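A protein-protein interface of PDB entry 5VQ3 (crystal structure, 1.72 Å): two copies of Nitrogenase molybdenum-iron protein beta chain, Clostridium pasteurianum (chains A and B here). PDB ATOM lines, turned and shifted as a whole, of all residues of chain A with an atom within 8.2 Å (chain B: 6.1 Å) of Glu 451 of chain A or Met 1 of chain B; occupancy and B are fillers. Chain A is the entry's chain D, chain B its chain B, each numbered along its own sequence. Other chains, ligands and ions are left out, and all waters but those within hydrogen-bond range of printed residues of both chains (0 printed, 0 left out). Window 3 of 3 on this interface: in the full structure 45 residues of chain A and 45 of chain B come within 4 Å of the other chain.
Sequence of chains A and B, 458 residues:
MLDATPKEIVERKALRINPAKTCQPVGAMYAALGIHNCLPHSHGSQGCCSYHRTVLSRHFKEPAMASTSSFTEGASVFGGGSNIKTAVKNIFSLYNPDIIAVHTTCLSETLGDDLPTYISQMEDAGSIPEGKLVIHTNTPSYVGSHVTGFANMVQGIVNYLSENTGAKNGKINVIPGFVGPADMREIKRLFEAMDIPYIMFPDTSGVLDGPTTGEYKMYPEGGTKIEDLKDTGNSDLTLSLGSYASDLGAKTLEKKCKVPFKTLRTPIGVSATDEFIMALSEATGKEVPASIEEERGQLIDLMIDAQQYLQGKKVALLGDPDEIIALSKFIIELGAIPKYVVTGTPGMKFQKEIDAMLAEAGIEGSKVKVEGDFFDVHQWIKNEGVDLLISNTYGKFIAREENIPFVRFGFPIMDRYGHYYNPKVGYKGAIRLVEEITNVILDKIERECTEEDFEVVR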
ATOM      1  N   GLU A 446     -10.674   6.191  10.816  1.00  0.00           N
ATOM      2  CA  GLU A 446     -11.894   6.787  11.392  1.00  0.00           C
ATOM      3  C   GLU A 446     -12.339   8.051  10.676  1.00  0.00           C
ATOM      4  O   GLU A 446     -13.516   8.423  10.745  1.00  0.00           O
ATOM      5  CB  GLU A 446     -11.753   7.030  12.904  1.00  0.00           C
ATOM      6  CG  GLU A 446     -11.397   5.719  13.611  1.00  0.00           C
ATOM      7  CD  GLU A 446     -11.751   5.686  15.088  1.00  0.00           C
ATOM      8  OE1 GLU A 446     -11.209   6.501  15.802  1.00  0.00           O
ATOM      9  OE2 GLU A 446     -12.553   4.820  15.516  1.00  0.00           O
ATOM     10  N   ARG A 447     -11.426   8.712   9.968  1.00  0.00           N
ATOM     11  CA  ARG A 447     -11.786   9.896   9.193  1.00  0.00           C
ATOM     12  C   ARG A 447     -12.478   9.495   7.897  1.00  0.00           C
ATOM     13  O   ARG A 447     -13.421  10.167   7.466  1.00  0.00           O
ATOM     14  CB  ARG A 447     -10.540  10.708   8.872  1.00  0.00           C
ATOM     15  CG  ARG A 447     -10.782  12.002   8.110  1.00  0.00           C
ATOM     16  CD  ARG A 447      -9.740  13.088   8.413  1.00  0.00           C
ATOM     17  NE  ARG A 447      -8.488  12.596   8.999  1.00  0.00           N
ATOM     18  CZ  ARG A 447      -7.518  11.967   8.332  1.00  0.00           C
ATOM     19  NH1 ARG A 447      -6.420  11.546   8.980  1.00  0.00           N
ATOM     20  NH2 ARG A 447      -7.651  11.722   7.032  1.00  0.00           N
ATOM     21  N   GLU A 448     -12.050   8.382   7.324  1.00  0.00           N
ATOM     22  CA  GLU A 448     -12.427   7.965   5.980  1.00  0.00           C
ATOM     23  C   GLU A 448     -13.475   6.863   5.900  1.00  0.00           C
ATOM     24  O   GLU A 448     -14.021   6.609   4.811  1.00  0.00           O
ATOM     25  CB  GLU A 448     -11.176   7.514   5.220  1.00  0.00           C
ATOM     26  CG  GLU A 448     -10.335   8.721   4.882  1.00  0.00           C
ATOM     27  CD  GLU A 448      -9.169   8.431   3.970  1.00  0.00           C
ATOM     28  OE1 GLU A 448      -8.983   7.255   3.564  1.00  0.00           O
ATOM     29  OE2 GLU A 448      -8.439   9.408   3.681  1.00  0.00           O
ATOM     30  N   CYS A 449     -13.752   6.181   6.998  1.00  0.00           N
ATOM     31  CA  CYS A 449     -14.739   5.092   6.939  1.00  0.00           C
ATOM     32  C   CYS A 449     -16.128   5.681   6.674  1.00  0.00           C
ATOM     33  O   CYS A 449     -16.385   6.851   6.933  1.00  0.00           O
ATOM     34  CB  CYS A 449     -14.744   4.242   8.222  1.00  0.00           C
ATOM     35  SG  CYS A 449     -15.238   5.124   9.732  1.00  0.00           S
ATOM     36  N   THR A 450     -17.013   4.880   6.107  1.00  0.00           N
ATOM     37  CA  THR A 450     -18.399   5.304   5.969  1.00  0.00           C
ATOM     38  C   THR A 450     -18.994   5.479   7.359  1.00  0.00           C
ATOM     39  O   THR A 450     -18.532   4.859   8.351  1.00  0.00           O
ATOM     40  CB  THR A 450     -19.255   4.272   5.226  1.00  0.00           C
ATOM     41  OG1 THR A 450     -19.207   3.027   5.943  1.00  0.00           O
ATOM     42  CG2 THR A 450     -18.733   4.072   3.824  1.00  0.00           C
ATOM     43  N   GLU A 451     -20.023   6.313   7.449  1.00  0.00           N
ATOM     44  CA  GLU A 451     -20.687   6.489   8.748  1.00  0.00           C
ATOM     45  C   GLU A 451     -21.157   5.170   9.368  1.00  0.00           C
ATOM     46  O   GLU A 451     -21.036   4.984  10.588  1.00  0.00           O
ATOM     47  CB  GLU A 451     -21.851   7.453   8.681  1.00  0.00           C
ATOM     48  CG  GLU A 451     -21.416   8.852   8.290  1.00  0.00           C
ATOM     49  CD  GLU A 451     -22.425   9.938   8.649  1.00  0.00           C
ATOM     50  OE1 GLU A 451     -23.583   9.637   9.046  1.00  0.00           O
ATOM     51  OE2 GLU A 451     -22.026  11.109   8.582  1.00  0.00           O
ATOM     52  N   GLU A 452     -21.687   4.253   8.560  1.00  0.00           N
ATOM     53  CA  GLU A 452     -22.188   2.988   9.137  1.00  0.00           C
ATOM     54  C   GLU A 452     -21.034   2.100   9.692  1.00  0.00           C
ATOM     55  O   GLU A 452     -21.264   1.239  10.536  1.00  0.00           O
ATOM     56  CB  GLU A 452     -23.072   2.236   8.106  1.00  0.00           C
ATOM     57  CG  GLU A 452     -22.316   1.734   6.877  1.00  0.00           C
ATOM     58  CD  GLU A 452     -22.387   2.697   5.699  1.00  0.00           C
ATOM     59  OE1 GLU A 452     -22.610   3.927   5.885  1.00  0.00           O
ATOM     60  OE2 GLU A 452     -22.210   2.219   4.568  1.00  0.00           O
ATOM     61  N   ASP A 453     -19.788   2.349   9.261  1.00  0.00           N
ATOM     62  CA  ASP A 453     -18.630   1.568   9.698  1.00  0.00           C
ATOM     63  C   ASP A 453     -17.870   2.231  10.832  1.00  0.00           C
ATOM     64  O   ASP A 453     -16.838   1.751  11.260  1.00  0.00           O
ATOM     65  CB  ASP A 453     -17.645   1.339   8.531  1.00  0.00           C
ATOM     66  CG  ASP A 453     -18.170   0.326   7.509  1.00  0.00           C
ATOM     67  OD1 ASP A 453     -19.176  -0.343   7.797  1.00  0.00           O
ATOM     68  OD2 ASP A 453     -17.571   0.207   6.414  1.00  0.00           O
ATOM     69  N   PHE A 454     -18.357   3.364  11.283  1.00  0.00           N
ATOM     70  CA  PHE A 454     -17.762   4.066  12.386  1.00  0.00           C
ATOM     71  C   PHE A 454     -18.016   3.282  13.673  1.00  0.00           C
ATOM     72  O   PHE A 454     -19.056   2.610  13.828  1.00  0.00           O
ATOM     73  CB  PHE A 454     -18.367   5.448  12.392  1.00  0.00           C
ATOM     74  CG  PHE A 454     -17.588   6.461  13.163  1.00  0.00           C
ATOM     75  CD1 PHE A 454     -16.482   7.116  12.601  1.00  0.00           C
ATOM     76  CD2 PHE A 454     -18.011   6.833  14.424  1.00  0.00           C
ATOM     77  CE1 PHE A 454     -15.799   8.106  13.295  1.00  0.00           C
ATOM     78  CE2 PHE A 454     -17.335   7.847  15.123  1.00  0.00           C
ATOM     79  CZ  PHE A 454     -16.224   8.464  14.553  1.00  0.00           C
ATOM     80  N   GLU A 455     -17.045   3.329  14.581  1.00  0.00           N
ATOM     81  CA  GLU A 455     -16.940   2.387  15.724  1.00  0.00           C
ATOM     82  C   GLU A 455     -16.684   3.163  16.994  1.00  0.00           C
ATOM     83  O   GLU A 455     -16.008   4.189  16.947  1.00  0.00           O
ATOM     84  CB  GLU A 455     -15.684   1.490  15.555  1.00  0.00           C
ATOM     85  CG  GLU A 455     -15.627   0.612  14.322  1.00  0.00           C
ATOM     86  CD  GLU A 455     -16.700  -0.466  14.302  1.00  0.00           C
ATOM     87  OE1 GLU A 455     -17.219  -0.795  15.383  1.00  0.00           O
ATOM     88  OE2 GLU A 455     -17.040  -0.951  13.197  1.00  0.00           O
ATOM     89  N   MET B   1     -23.560  12.494  10.411  1.00  0.00           N
ATOM     90  CA  MET B   1     -23.380  11.739  11.675  1.00  0.00           C
ATOM     91  C   MET B   1     -24.144  12.524  12.750  1.00  0.00           C
ATOM     92  O   MET B   1     -24.196  13.755  12.678  1.00  0.00           O
ATOM     93  CB  MET B   1     -21.870  11.632  11.981  1.00  0.00           C
ATOM     94  CG  MET B   1     -21.505  11.077  13.347  1.00  0.00           C
ATOM     95  SD  MET B   1     -19.802  10.424  13.382  1.00  0.00           S
ATOM     96  CE  MET B   1     -20.009   9.008  12.257  1.00  0.00           C
ATOM     97  N   LEU B   2     -24.717  11.815  13.728  1.00  0.00           N
ATOM     98  CA  LEU B   2     -25.551  12.434  14.759  1.00  0.00           C
ATOM     99  C   LEU B   2     -26.578  13.331  14.066  1.00  0.00           C
ATOM    100  O   LEU B   2     -26.848  14.486  14.446  1.00  0.00           O
ATOM    101  CB  LEU B   2     -24.703  13.180  15.782  1.00  0.00           C
ATOM    102  CG  LEU B   2     -23.777  12.330  16.672  1.00  0.00           C
ATOM    103  CD1 LEU B   2     -22.768  13.241  17.382  1.00  0.00           C
ATOM    104  CD2 LEU B   2     -24.552  11.524  17.697  1.00  0.00           C
ATOM    105  N   ASP B   3     -27.182  12.779  13.023  1.00  0.00           N
ATOM    106  CA  ASP B   3     -28.063  13.601  12.173  1.00  0.00           C
ATOM    107  C   ASP B   3     -29.336  14.018  12.888  1.00  0.00           C
ATOM    108  O   ASP B   3     -29.957  15.029  12.544  1.00  0.00           O
ATOM    109  CB  ASP B   3     -28.425  12.841  10.910  1.00  0.00           C
ATOM    110  CG  ASP B   3     -27.252  12.666   9.957  1.00  0.00           C
ATOM    111  OD1 ASP B   3     -26.203  13.326  10.120  1.00  0.00           O
ATOM    112  OD2 ASP B   3     -27.399  11.854   9.014  1.00  0.00           O
ATOM    113  N   ALA B   4     -29.726  13.267  13.908  1.00  0.00           N
ATOM    114  CA  ALA B   4     -30.952  13.584  14.647  1.00  0.00           C
ATOM    115  C   ALA B   4     -30.830  14.730  15.681  1.00  0.00           C
ATOM    116  O   ALA B   4     -31.793  15.091  16.346  1.00  0.00           O
ATOM    117  CB  ALA B   4     -31.460  12.320  15.300  1.00  0.00           C
ATOM    118  N   HIS B 378     -23.066  19.095  21.862  1.00  0.00           N
ATOM    119  CA  HIS B 378     -23.208  19.099  20.446  1.00  0.00           C
ATOM    120  C   HIS B 378     -24.150  20.226  19.989  1.00  0.00           C
ATOM    121  O   HIS B 378     -23.794  21.004  19.116  1.00  0.00           O
ATOM    122  CB  HIS B 378     -23.632  17.731  19.923  1.00  0.00           C
ATOM    123  CG  HIS B 378     -23.523  17.620  18.452  1.00  0.00           C
ATOM    124  ND1 HIS B 378     -24.107  16.597  17.743  1.00  0.00           N
ATOM    125  CD2 HIS B 378     -22.888  18.402  17.544  1.00  0.00           C
ATOM    126  CE1 HIS B 378     -23.884  16.781  16.455  1.00  0.00           C
ATOM    127  NE2 HIS B 378     -23.143  17.863  16.310  1.00  0.00           N
ATOM    128  N   LYS B 396     -15.816  11.448  19.949  1.00  0.00           N
ATOM    129  CA  LYS B 396     -15.316  11.252  18.591  1.00  0.00           C
ATOM    130  C   LYS B 396     -16.446  11.493  17.556  1.00  0.00           C
ATOM    131  O   LYS B 396     -16.176  11.831  16.424  1.00  0.00           O
ATOM    132  CB  LYS B 396     -14.727   9.844  18.445  1.00  0.00           C
ATOM    133  CG  LYS B 396     -15.762   8.743  18.450  1.00  0.00           C
ATOM    134  CD  LYS B 396     -15.174   7.337  18.671  1.00  0.00           C
ATOM    135  CE  LYS B 396     -14.403   6.859  17.479  1.00  0.00           C
ATOM    136  NZ  LYS B 396     -13.788   5.544  17.761  1.00  0.00           N
ATOM    137  N   PHE B 397     -17.694  11.287  17.950  1.00  0.00           N
ATOM    138  CA  PHE B 397     -18.800  11.390  16.979  1.00  0.00           C
ATOM    139  C   PHE B 397     -19.003  12.871  16.679  1.00  0.00           C
ATOM    140  O   PHE B 397     -19.244  13.242  15.552  1.00  0.00           O
ATOM    141  CB  PHE B 397     -20.078  10.822  17.532  1.00  0.00           C
ATOM    142  CG  PHE B 397     -20.047   9.312  17.719  1.00  0.00           C
ATOM    143  CD1 PHE B 397     -19.493   8.760  18.840  1.00  0.00           C
ATOM    144  CD2 PHE B 397     -20.516   8.484  16.746  1.00  0.00           C
ATOM    145  CE1 PHE B 397     -19.455   7.381  19.015  1.00  0.00           C
ATOM    146  CE2 PHE B 397     -20.494   7.121  16.883  1.00  0.00           C
ATOM    147  CZ  PHE B 397     -19.963   6.561  18.037  1.00  0.00           C
ATOM    148  N   ILE B 398     -18.926  13.680  17.722  1.00  0.00           N
ATOM    149  CA  ILE B 398     -19.002  15.143  17.578  1.00  0.00           C
ATOM    150  C   ILE B 398     -17.822  15.659  16.788  1.00  0.00           C
ATOM    151  O   ILE B 398     -17.979  16.485  15.889  1.00  0.00           O
ATOM    152  CB  ILE B 398     -19.095  15.847  18.936  1.00  0.00           C
ATOM    153  CG1 ILE B 398     -20.394  15.459  19.659  1.00  0.00           C
ATOM    154  CG2 ILE B 398     -19.013  17.366  18.800  1.00  0.00           C
ATOM    155  CD1 ILE B 398     -20.431  15.954  21.100  1.00  0.00           C
ATOM    156  N   ARG B 400     -15.983  14.183  14.529  1.00  0.00           N
ATOM    157  CA  ARG B 400     -16.094  13.925  13.125  1.00  0.00           C
ATOM    158  C   ARG B 400     -17.209  14.742  12.486  1.00  0.00           C
ATOM    159  O   ARG B 400     -17.003  15.337  11.454  1.00  0.00           O
ATOM    160  CB  ARG B 400     -16.354  12.465  12.859  1.00  0.00           C
ATOM    161  CG  ARG B 400     -16.717  12.212  11.391  1.00  0.00           C
ATOM    162  CD  ARG B 400     -16.432  10.799  10.976  1.00  0.00           C
ATOM    163  NE  ARG B 400     -17.172  10.520   9.750  1.00  0.00           N
ATOM    164  CZ  ARG B 400     -16.892   9.515   8.940  1.00  0.00           C
ATOM    165  NH1 ARG B 400     -15.916   8.690   9.251  1.00  0.00           N
ATOM    166  NH2 ARG B 400     -17.623   9.315   7.850  1.00  0.00           N
ATOM    167  N   GLU B 401     -18.380  14.773  13.105  1.00  0.00           N
ATOM    168  CA  GLU B 401     -19.501  15.491  12.502  1.00  0.00           C
ATOM    169  C   GLU B 401     -19.215  16.991  12.329  1.00  0.00           C
ATOM    170  O   GLU B 401     -19.598  17.582  11.321  1.00  0.00           O
ATOM    171  CB  GLU B 401     -20.747  15.304  13.333  1.00  0.00           C
ATOM    172  CG  GLU B 401     -21.915  16.196  12.963  1.00  0.00           C
ATOM    173  CD  GLU B 401     -22.569  15.876  11.609  1.00  0.00           C
ATOM    174  OE1 GLU B 401     -22.094  14.995  10.846  1.00  0.00           O
ATOM    175  OE2 GLU B 401     -23.587  16.537  11.307  1.00  0.00           O
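Among the printed residues, 11 pairs touch across the chains.
Glu 451 of chain A touches two residues of chain B. Of the printed residues of chain B, Phe 454 of chain A touches Met 1 (3.6 Å), Lys 396 (3.8 Å), Phe 397 (3.5 Å) and Arg 400 (3.6 Å). Printed residues of chain B within 4 Å of Glu 455 of chain A: Lys 396. Of the printed residues of chain A, Lys 396 of chain B touches Glu 446 (2.7 Å), Phe 454 (3.8 Å) and Glu 455 (2.7 Å). Of the printed residues of chain A, Phe 397 of chain B touches Phe 454. Printed residues of chain A within 4 Å of Arg 400 of chain B: Glu 446 (2.8 Å), Arg 447 (3.4 Å), Cys 449 (2.9 Å), Glu 451 (3.8 Å) and Phe 454 (3.6 Å). The nearest residue of chain B that does not touch Glu 451 of chain A is Asp 3 of chain B (4.4 Å). The nearest residue of chain A that does not touch Met 1 of chain B is Thr 450 of chain A (5.9 Å).
The side-chain carboxylate (OE2) of Glu 451 of chain A lies within hydrogen-bond range of the backbone NH (N) of Met 1 of chain B, at 2.8 Å. The side-chain carboxylate (OE2) of Glu 446 of chain A lies within salt-bridge range of the side-chain amino group (NZ) of Lys 396 of chain B (2.7 Å). The backbone carbonyl oxygen (O) of Glu 455 of chain A sits at hydrogen-bond distance from the side-chain amino group (NZ) of Lys 396 of chain B (2.7 Å). O of Glu 446 of chain A is in hydrogen-bond range of NH1 of Arg 400 of chain B (2.8 Å). NH1 of Arg 400 of chain B sits at hydrogen-bond distance from O of Arg 447 of chain A (3.4 Å). O of Cys 449 of chain A is in hydrogen-bond range of NH2 of Arg 400 of chain B (2.9 Å).
Among the printed residues, merely in contact across the chains: Phe 454 of chain A with Phe 397 of chain B (3.5 Å), Phe 454 of chain A with Arg 400 of chain B (3.6 Å), Phe 454 of chain A with Met 1 of chain B (3.6 Å), Phe 454 of chain A with Lys 396 of chain B (3.8 Å) and Glu 451 of chain A with Arg 400 of chain B (3.8 Å).
The side-chain carboxylate (OD1) of Asp 3 of chain B lies within hydrogen-bond range of the backbone NH (N) of Met 1 of chain B (2.8 Å). The backbone NH (N) of Met 1 of chain B lies within hydrogen-bond range of the side-chain carboxylate (OE1) of Glu 401 of chain B (2.9 Å).
No position is printed for both chains. Of the 11 pairs that touch across the chains among the printed residues, none has its exchanged pair printed and touching as well.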
